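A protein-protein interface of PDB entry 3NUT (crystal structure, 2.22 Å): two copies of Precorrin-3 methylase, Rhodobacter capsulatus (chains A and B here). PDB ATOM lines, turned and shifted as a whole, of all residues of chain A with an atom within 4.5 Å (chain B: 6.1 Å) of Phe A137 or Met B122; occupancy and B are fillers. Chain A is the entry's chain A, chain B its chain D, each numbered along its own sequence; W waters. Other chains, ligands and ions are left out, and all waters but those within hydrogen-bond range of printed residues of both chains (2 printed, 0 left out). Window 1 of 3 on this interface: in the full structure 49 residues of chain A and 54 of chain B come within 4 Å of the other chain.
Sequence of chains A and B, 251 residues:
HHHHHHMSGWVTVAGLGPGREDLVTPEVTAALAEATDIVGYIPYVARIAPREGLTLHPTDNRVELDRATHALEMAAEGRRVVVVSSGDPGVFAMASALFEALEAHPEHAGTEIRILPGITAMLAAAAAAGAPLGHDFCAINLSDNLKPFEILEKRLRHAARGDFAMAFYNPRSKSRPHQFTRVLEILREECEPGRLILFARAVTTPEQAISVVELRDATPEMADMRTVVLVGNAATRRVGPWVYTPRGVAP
The backbone carbonyl oxygen (O) of Phe A137 lies within hydrogen-bond range of the backbone NH (N) of Ala B139 (2.8 Å).
O of Leu A133 lies close to O of Gly B90 (3.2 Å).
The backbone NH (N) of Ala A165 lies within hydrogen-bond range of the backbone carbonyl oxygen (O) of Asp A136 (3.1 Å).
The backbone carbonyl oxygen (O) of Ala A165 lies within hydrogen-bond range of the backbone NH (N) of Cys A138 (2.9 Å).
OG1 of Thr B120 sits at hydrogen-bond distance from OH of Tyr B169.
The backbone carbonyl oxygen (O) of Cys B138 is in hydrogen-bond range of the backbone NH (N) of Ala B167 (2.8 Å).
O of Ala B167 sits at hydrogen-bond distance from N of Ile B140, at 2.8 Å.
The backbone carbonyl oxygen of Ile B140 sits at hydrogen-bond distance from the backbone NH of Tyr B169 (3.0 Å).
Among the printed residues, merely in contact across the chains: Cys A138 with Phe B137 (3.2 Å), Phe A137 with Cys B138 (3.2 Å), Asp A136 with Ala B139 (3.4 Å), Asp A136 with Ile B140 (3.4 Å), Asp A136 with Phe B92 (3.4 Å), Phe A164 with Ile B140 (3.5 Å), Phe A137 with Met B122 (3.6 Å), Cys A138 with Cys B138 (3.7 Å), Leu A123 with Val B91 (3.8 Å), Phe A164 with Cys B138 (3.8 Å), His A135 with Phe B92 (3.8 Å) and Leu A123 with Thr B120 (3.9 Å).
Of the printed residues of chain B, Asp A136 touches Phe B92 (3.4 Å), Ala B139 (3.4 Å) and Ile B140 (3.4 Å).
Of chain B, only Met B122 (3.6 Å), Cys B138 (3.2 Å) and Ala B139 (2.8 Å) come within 4 Å of Phe A137.
Of the printed residues of chain B, Cys A138 touches Phe B137 (3.2 Å) and Cys B138 (3.7 Å).
Of the printed residues of chain A, Val B91 touches Leu A123.
Met B122 touches just one residue of chain A: Phe A137 (3.6 Å).
Printed residues of chain A within 4 Å of Ile B140: Asp A136 (3.4 Å) and Phe A164 (3.5 Å).
The nearest residue of chain B that does not touch Phe A137 is Val B91 (4.4 Å).
The nearest printed residue of chain A that does not touch Met B122 is Leu A123 (5.4 Å).
The nearest printed residue of chain A that does not touch Phe B92 is Leu A133 (5.0 Å).
Hydrophobic or aromatic side chains of chain A within 4 Å of the printed part of chain B: Leu A123, Phe A137 and Phe A164.
Of the 20 printed residues of chain B, 9 touch a printed residue of chain A.
Printed residues of chain B that touch a printed residue of chain A: Gly B90, Val B91, Phe B92, Thr B120, Met B122, Phe B137, Cys B138, Ala B139 and Ile B140.
Hydrophobic or aromatic side chains of chain B that line the printed part of chain A: Val B91, Phe B92, Met B122, Ala B139 and Ile B140.
Among the printed residues, 14 pairs touch across the chains.
Phe A137 touches Met B122, but with the chains exchanged Met A122 does not touch Phe B137 (4.9 Å).
Phe A137 touches Cys B138, and with the chains exchanged Cys A138 touches Phe B137.
Cys A138 touches its own counterpart, Cys B138.
Positions printed for both chains: 122, 123, 133, 137 and 138.
Of the 14 pairs that touch across the chains among the printed residues, 3 have their exchanged pair printed and touching as well.
Water W2 bridges the backbone carbonyl oxygen of Leu A133 (2.7 Å) and the backbone NH of Phe B92 (3.0 Å).
Water W1 bridges N of Leu A133 (2.8 Å) and O of Gly B90 (3.3 Å).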
ATOM      1  N   MET A 122      31.299  29.591   9.000  1.00  0.00           N
ATOM      2  CA  MET A 122      32.347  28.735   9.577  1.00  0.00           C
ATOM      3  C   MET A 122      32.381  27.330   8.955  1.00  0.00           C
ATOM      4  O   MET A 122      33.442  26.830   8.556  1.00  0.00           O
ATOM      5  CB  MET A 122      32.247  28.652  11.108  1.00  0.00           C
ATOM      6  CG  MET A 122      31.016  27.932  11.678  1.00  0.00           C
ATOM      7  SD  MET A 122      30.998  27.989  13.500  1.00  0.00           S
ATOM      8  CE  MET A 122      32.494  27.082  13.852  1.00  0.00           C
ATOM      9  N   LEU A 123      31.199  26.729   8.857  1.00  0.00           N
ATOM     10  CA  LEU A 123      31.042  25.376   8.350  1.00  0.00           C
ATOM     11  C   LEU A 123      31.189  25.361   6.847  1.00  0.00           C
ATOM     12  O   LEU A 123      31.608  24.363   6.297  1.00  0.00           O
ATOM     13  CB  LEU A 123      29.684  24.786   8.777  1.00  0.00           C
ATOM     14  CG  LEU A 123      29.479  24.455  10.273  1.00  0.00           C
ATOM     15  CD1 LEU A 123      28.194  23.683  10.453  1.00  0.00           C
ATOM     16  CD2 LEU A 123      30.623  23.648  10.856  1.00  0.00           C
ATOM     17  N   LEU A 133      36.939  21.703  11.854  1.00  0.00           N
ATOM     18  CA  LEU A 133      36.076  21.784  13.022  1.00  0.00           C
ATOM     19  C   LEU A 133      35.448  20.427  13.290  1.00  0.00           C
ATOM     20  O   LEU A 133      34.361  20.313  13.888  1.00  0.00           O
ATOM     21  CB  LEU A 133      34.991  22.863  12.827  1.00  0.00           C
ATOM     22  CG  LEU A 133      35.471  24.284  12.570  1.00  0.00           C
ATOM     23  CD1 LEU A 133      34.418  25.060  11.800  1.00  0.00           C
ATOM     24  CD2 LEU A 133      35.863  25.016  13.851  1.00  0.00           C
ATOM     25  N   HIS A 135      36.332  18.223  15.386  1.00  0.00           N
ATOM     26  CA  HIS A 135      36.248  17.937  16.811  1.00  0.00           C
ATOM     27  C   HIS A 135      35.534  19.083  17.517  1.00  0.00           C
ATOM     28  O   HIS A 135      35.168  20.059  16.870  1.00  0.00           O
ATOM     29  CB  HIS A 135      37.651  17.764  17.398  1.00  0.00           C
ATOM     30  CG  HIS A 135      38.232  16.399  17.187  1.00  0.00           C
ATOM     31  ND1 HIS A 135      38.276  15.789  15.946  1.00  0.00           N
ATOM     32  CD2 HIS A 135      38.815  15.534  18.056  1.00  0.00           C
ATOM     33  CE1 HIS A 135      38.848  14.604  16.065  1.00  0.00           C
ATOM     34  NE2 HIS A 135      39.189  14.428  17.332  1.00  0.00           N
ATOM     35  N   ASP A 136      35.353  18.946  18.837  1.00  0.00           N
ATOM     36  CA  ASP A 136      34.831  20.003  19.699  1.00  0.00           C
ATOM     37  C   ASP A 136      35.351  21.372  19.281  1.00  0.00           C
ATOM     38  O   ASP A 136      36.560  21.572  19.119  1.00  0.00           O
ATOM     39  CB  ASP A 136      35.193  19.732  21.157  1.00  0.00           C
ATOM     40  CG  ASP A 136      34.579  18.445  21.679  1.00  0.00           C
ATOM     41  OD1 ASP A 136      33.882  17.763  20.909  1.00  0.00           O
ATOM     42  OD2 ASP A 136      34.790  18.106  22.859  1.00  0.00           O
ATOM     43  N   PHE A 137      34.431  22.304  19.065  1.00  0.00           N
ATOM     44  CA  PHE A 137      34.802  23.626  18.582  1.00  0.00           C
ATOM     45  C   PHE A 137      33.876  24.693  19.147  1.00  0.00           C
ATOM     46  O   PHE A 137      32.811  24.389  19.699  1.00  0.00           O
ATOM     47  CB  PHE A 137      34.809  23.646  17.038  1.00  0.00           C
ATOM     48  CG  PHE A 137      33.434  23.531  16.416  1.00  0.00           C
ATOM     49  CD1 PHE A 137      32.663  24.668  16.187  1.00  0.00           C
ATOM     50  CD2 PHE A 137      32.917  22.290  16.069  1.00  0.00           C
ATOM     51  CE1 PHE A 137      31.388  24.568  15.612  1.00  0.00           C
ATOM     52  CE2 PHE A 137      31.629  22.179  15.506  1.00  0.00           C
ATOM     53  CZ  PHE A 137      30.874  23.326  15.267  1.00  0.00           C
ATOM     54  N   CYS A 138      34.274  25.946  19.004  1.00  0.00           N
ATOM     55  CA  CYS A 138      33.405  27.038  19.427  1.00  0.00           C
ATOM     56  C   CYS A 138      33.382  28.170  18.414  1.00  0.00           C
ATOM     57  O   CYS A 138      34.301  28.310  17.601  1.00  0.00           O
ATOM     58  CB  CYS A 138      33.842  27.555  20.790  1.00  0.00           C
ATOM     59  SG  CYS A 138      35.472  28.284  20.760  1.00  0.00           S
ATOM     60  N   PHE A 164      39.525  23.562  22.630  1.00  0.00           N
ATOM     61  CA  PHE A 164      38.501  23.714  21.596  1.00  0.00           C
ATOM     62  C   PHE A 164      39.138  24.256  20.319  1.00  0.00           C
ATOM     63  O   PHE A 164      39.949  25.188  20.368  1.00  0.00           O
ATOM     64  CB  PHE A 164      37.469  24.749  22.048  1.00  0.00           C
ATOM     65  CG  PHE A 164      36.486  24.241  23.055  1.00  0.00           C
ATOM     66  CD1 PHE A 164      35.352  23.572  22.652  1.00  0.00           C
ATOM     67  CD2 PHE A 164      36.688  24.457  24.404  1.00  0.00           C
ATOM     68  CE1 PHE A 164      34.420  23.111  23.588  1.00  0.00           C
ATOM     69  CE2 PHE A 164      35.768  23.989  25.347  1.00  0.00           C
ATOM     70  CZ  PHE A 164      34.632  23.310  24.932  1.00  0.00           C
ATOM     71  N   ALA A 165      38.739  23.713  19.178  1.00  0.00           N
ATOM     72  CA  ALA A 165      39.038  24.373  17.925  1.00  0.00           C
ATOM     73  C   ALA A 165      38.147  25.615  17.923  1.00  0.00           C
ATOM     74  O   ALA A 165      37.185  25.687  18.700  1.00  0.00           O
ATOM     75  CB  ALA A 165      38.748  23.440  16.717  1.00  0.00           C
ATOM     76  N   GLY B  90      31.182  18.086   8.254  1.00  0.00           N
ATOM     77  CA  GLY B  90      32.264  18.518   9.145  1.00  0.00           C
ATOM     78  C   GLY B  90      32.002  18.555  10.655  1.00  0.00           C
ATOM     79  O   GLY B  90      32.875  19.002  11.411  1.00  0.00           O
ATOM     80  N   VAL B  91      30.825  18.117  11.099  1.00  0.00           N
ATOM     81  CA  VAL B  91      30.449  18.181  12.521  1.00  0.00           C
ATOM     82  C   VAL B  91      30.294  16.754  13.071  1.00  0.00           C
ATOM     83  O   VAL B  91      29.230  16.121  12.928  1.00  0.00           O
ATOM     84  CB  VAL B  91      29.125  18.994  12.756  1.00  0.00           C
ATOM     85  CG1 VAL B  91      28.660  18.925  14.213  1.00  0.00           C
ATOM     86  CG2 VAL B  91      29.269  20.447  12.283  1.00  0.00           C
ATOM     87  N   PHE B  92      31.370  16.257  13.689  1.00  0.00           N
ATOM     88  CA  PHE B  92      31.402  14.892  14.257  1.00  0.00           C
ATOM     89  C   PHE B  92      30.939  13.866  13.213  1.00  0.00           C
ATOM     90  O   PHE B  92      30.156  12.984  13.517  1.00  0.00           O
ATOM     91  CB  PHE B  92      30.513  14.806  15.515  1.00  0.00           C
ATOM     92  CG  PHE B  92      30.739  15.915  16.512  1.00  0.00           C
ATOM     93  CD1 PHE B  92      32.024  16.156  17.045  1.00  0.00           C
ATOM     94  CD2 PHE B  92      29.675  16.691  16.940  1.00  0.00           C
ATOM     95  CE1 PHE B  92      32.245  17.160  17.967  1.00  0.00           C
ATOM     96  CE2 PHE B  92      29.864  17.714  17.878  1.00  0.00           C
ATOM     97  CZ  PHE B  92      31.158  17.946  18.405  1.00  0.00           C
ATOM     98  N   THR B 120      23.325  21.926  10.254  1.00  0.00           N
ATOM     99  CA  THR B 120      23.723  21.057  11.311  1.00  0.00           C
ATOM    100  C   THR B 120      22.636  21.034  12.392  1.00  0.00           C
ATOM    101  O   THR B 120      21.856  21.967  12.493  1.00  0.00           O
ATOM    102  CB  THR B 120      25.112  21.418  11.834  1.00  0.00           C
ATOM    103  OG1 THR B 120      25.569  20.336  12.651  1.00  0.00           O
ATOM    104  CG2 THR B 120      25.075  22.724  12.648  1.00  0.00           C
ATOM    105  N   ALA B 121      22.610  19.963  13.181  1.00  0.00           N
ATOM    106  CA  ALA B 121      21.545  19.686  14.158  1.00  0.00           C
ATOM    107  C   ALA B 121      21.315  20.764  15.208  1.00  0.00           C
ATOM    108  O   ALA B 121      20.161  21.115  15.509  1.00  0.00           O
ATOM    109  CB  ALA B 121      21.807  18.373  14.849  1.00  0.00           C
ATOM    110  N   MET B 122      22.399  21.258  15.780  1.00  0.00           N
ATOM    111  CA  MET B 122      22.307  22.303  16.795  1.00  0.00           C
ATOM    112  C   MET B 122      21.611  23.562  16.270  1.00  0.00           C
ATOM    113  O   MET B 122      20.809  24.149  16.982  1.00  0.00           O
ATOM    114  CB  MET B 122      23.667  22.650  17.413  1.00  0.00           C
ATOM    115  CG  MET B 122      24.708  23.156  16.425  1.00  0.00           C
ATOM    116  SD  MET B 122      26.266  23.619  17.212  1.00  0.00           S
ATOM    117  CE  MET B 122      27.322  23.604  15.741  1.00  0.00           C
ATOM    118  N   LEU B 123      21.870  23.933  15.022  1.00  0.00           N
ATOM    119  CA  LEU B 123      21.320  25.176  14.499  1.00  0.00           C
ATOM    120  C   LEU B 123      19.900  25.049  14.053  1.00  0.00           C
ATOM    121  O   LEU B 123      19.161  26.009  14.102  1.00  0.00           O
ATOM    122  CB  LEU B 123      22.155  25.713  13.361  1.00  0.00           C
ATOM    123  CG  LEU B 123      23.481  26.245  13.858  1.00  0.00           C
ATOM    124  CD1 LEU B 123      24.362  26.530  12.635  1.00  0.00           C
ATOM    125  CD2 LEU B 123      23.248  27.486  14.749  1.00  0.00           C
ATOM    126  N   ALA B 124      19.541  23.869  13.583  1.00  0.00           N
ATOM    127  CA  ALA B 124      18.157  23.517  13.327  1.00  0.00           C
ATOM    128  C   ALA B 124      17.364  23.527  14.657  1.00  0.00           C
ATOM    129  O   ALA B 124      16.229  23.987  14.717  1.00  0.00           O
ATOM    130  CB  ALA B 124      18.101  22.142  12.649  1.00  0.00           C
ATOM    131  N   ALA B 125      17.985  23.021  15.721  1.00  0.00           N
ATOM    132  CA  ALA B 125      17.365  23.003  17.057  1.00  0.00           C
ATOM    133  C   ALA B 125      17.183  24.424  17.581  1.00  0.00           C
ATOM    134  O   ALA B 125      16.099  24.791  18.051  1.00  0.00           O
ATOM    135  CB  ALA B 125      18.213  22.161  18.049  1.00  0.00           C
ATOM    136  N   ALA B 126      18.256  25.206  17.474  1.00  0.00           N
ATOM    137  CA  ALA B 126      18.263  26.617  17.841  1.00  0.00           C
ATOM    138  C   ALA B 126      17.139  27.323  17.138  1.00  0.00           C
ATOM    139  O   ALA B 126      16.332  28.017  17.779  1.00  0.00           O
ATOM    140  CB  ALA B 126      19.602  27.271  17.468  1.00  0.00           C
ATOM    141  N   ALA B 127      17.069  27.148  15.816  1.00  0.00           N
ATOM    142  CA  ALA B 127      16.019  27.823  15.057  1.00  0.00           C
ATOM    143  C   ALA B 127      14.624  27.443  15.556  1.00  0.00           C
ATOM    144  O   ALA B 127      13.708  28.261  15.517  1.00  0.00           O
ATOM    145  CB  ALA B 127      16.136  27.558  13.580  1.00  0.00           C
ATOM    146  N   LEU B 133      21.513  30.051  20.613  1.00  0.00           N
ATOM    147  CA  LEU B 133      22.931  30.011  20.243  1.00  0.00           C
ATOM    148  C   LEU B 133      23.372  31.351  19.670  1.00  0.00           C
ATOM    149  O   LEU B 133      24.387  31.447  18.993  1.00  0.00           O
ATOM    150  CB  LEU B 133      23.205  28.828  19.298  1.00  0.00           C
ATOM    151  CG  LEU B 133      22.893  27.433  19.866  1.00  0.00           C
ATOM    152  CD1 LEU B 133      23.487  26.295  18.994  1.00  0.00           C
ATOM    153  CD2 LEU B 133      23.418  27.293  21.298  1.00  0.00           C
ATOM    154  N   PHE B 137      29.221  30.313  21.371  1.00  0.00           N
ATOM    155  CA  PHE B 137      28.763  28.991  21.723  1.00  0.00           C
ATOM    156  C   PHE B 137      29.789  27.954  21.335  1.00  0.00           C
ATOM    157  O   PHE B 137      30.685  28.218  20.540  1.00  0.00           O
ATOM    158  CB  PHE B 137      27.397  28.696  21.068  1.00  0.00           C
ATOM    159  CG  PHE B 137      27.418  28.637  19.554  1.00  0.00           C
ATOM    160  CD1 PHE B 137      27.485  27.418  18.892  1.00  0.00           C
ATOM    161  CD2 PHE B 137      27.318  29.786  18.805  1.00  0.00           C
ATOM    162  CE1 PHE B 137      27.478  27.344  17.476  1.00  0.00           C
ATOM    163  CE2 PHE B 137      27.300  29.728  17.393  1.00  0.00           C
ATOM    164  CZ  PHE B 137      27.385  28.492  16.733  1.00  0.00           C
ATOM    165  N   CYS B 138      29.628  26.762  21.876  1.00  0.00           N
ATOM    166  CA  CYS B 138      30.523  25.668  21.540  1.00  0.00           C
ATOM    167  C   CYS B 138      29.740  24.400  21.274  1.00  0.00           C
ATOM    168  O   CYS B 138      28.567  24.282  21.661  1.00  0.00           O
ATOM    169  CB  CYS B 138      31.526  25.454  22.676  1.00  0.00           C
ATOM    170  SG  CYS B 138      30.799  24.779  24.139  1.00  0.00           S
ATOM    171  N   ALA B 139      30.378  23.456  20.602  1.00  0.00           N
ATOM    172  CA  ALA B 139      29.734  22.182  20.342  1.00  0.00           C
ATOM    173  C   ALA B 139      30.635  21.096  20.906  1.00  0.00           C
ATOM    174  O   ALA B 139      31.843  21.160  20.704  1.00  0.00           O
ATOM    175  CB  ALA B 139      29.504  21.990  18.821  1.00  0.00           C
ATOM    176  N   ILE B 140      30.054  20.114  21.603  1.00  0.00           N
ATOM    177  CA  ILE B 140      30.830  19.015  22.207  1.00  0.00           C
ATOM    178  C   ILE B 140      30.211  17.624  21.975  1.00  0.00           C
ATOM    179  O   ILE B 140      29.007  17.420  22.164  1.00  0.00           O
ATOM    180  CB  ILE B 140      31.097  19.253  23.732  1.00  0.00           C
ATOM    181  CG1 ILE B 140      32.038  20.438  23.933  1.00  0.00           C
ATOM    182  CG2 ILE B 140      31.747  18.043  24.358  1.00  0.00           C
ATOM    183  CD1 ILE B 140      31.738  21.287  25.184  1.00  0.00           C
ATOM    184  N   ALA B 167      26.262  23.094  22.836  1.00  0.00           N
ATOM    185  CA  ALA B 167      25.464  22.075  22.163  1.00  0.00           C
ATOM    186  C   ALA B 167      26.109  20.693  22.363  1.00  0.00           C
ATOM    187  O   ALA B 167      27.279  20.489  22.025  1.00  0.00           O
ATOM    188  CB  ALA B 167      25.322  22.412  20.689  1.00  0.00           C
ATOM    189  N   TYR B 169      26.204  16.886  21.224  1.00  0.00           N
ATOM    190  CA  TYR B 169      25.891  15.874  20.211  1.00  0.00           C
ATOM    191  C   TYR B 169      26.102  14.482  20.837  1.00  0.00           C
ATOM    192  O   TYR B 169      26.993  14.304  21.687  1.00  0.00           O
ATOM    193  CB  TYR B 169      26.786  16.061  18.958  1.00  0.00           C
ATOM    194  CG  TYR B 169      26.347  17.172  18.018  1.00  0.00           C
ATOM    195  CD1 TYR B 169      25.730  16.883  16.800  1.00  0.00           C
ATOM    196  CD2 TYR B 169      26.538  18.513  18.349  1.00  0.00           C
ATOM    197  CE1 TYR B 169      25.330  17.899  15.925  1.00  0.00           C
ATOM    198  CE2 TYR B 169      26.127  19.553  17.488  1.00  0.00           C
ATOM    199  CZ  TYR B 169      25.517  19.241  16.285  1.00  0.00           C
ATOM    200  OH  TYR B 169      25.114  20.260  15.439  1.00  0.00           O
ATOM    201  N   VAL B 228      19.637  16.556  20.486  1.00  0.00           N
ATOM    202  CA  VAL B 228      20.768  17.474  20.686  1.00  0.00           C
ATOM    203  C   VAL B 228      20.433  18.305  21.914  1.00  0.00           C
ATOM    204  O   VAL B 228      19.288  18.761  22.102  1.00  0.00           O
ATOM    205  CB  VAL B 228      21.091  18.361  19.428  1.00  0.00           C
ATOM    206  CG1 VAL B 228      19.942  19.270  19.059  1.00  0.00           C
ATOM    207  CG2 VAL B 228      22.362  19.179  19.638  1.00  0.00           C
ATOM    208  N   LEU B 230      20.881  21.568  23.996  1.00  0.00           N
ATOM    209  CA  LEU B 230      21.392  22.926  23.999  1.00  0.00           C
ATOM    210  C   LEU B 230      21.460  23.474  25.411  1.00  0.00           C
ATOM    211  O   LEU B 230      20.519  23.323  26.213  1.00  0.00           O
ATOM    212  CB  LEU B 230      20.534  23.842  23.111  1.00  0.00           C
ATOM    213  CG  LEU B 230      20.284  23.413  21.656  1.00  0.00           C
ATOM    214  CD1 LEU B 230      19.654  24.542  20.849  1.00  0.00           C
ATOM    215  CD2 LEU B 230      21.590  22.942  20.991  1.00  0.00           C
HETATM  216  O   HOH W   1      35.276  20.579   9.835  1.00  0.00           O
HETATM  217  O   HOH W   2      32.508  18.678  15.005  1.00  0.00           O
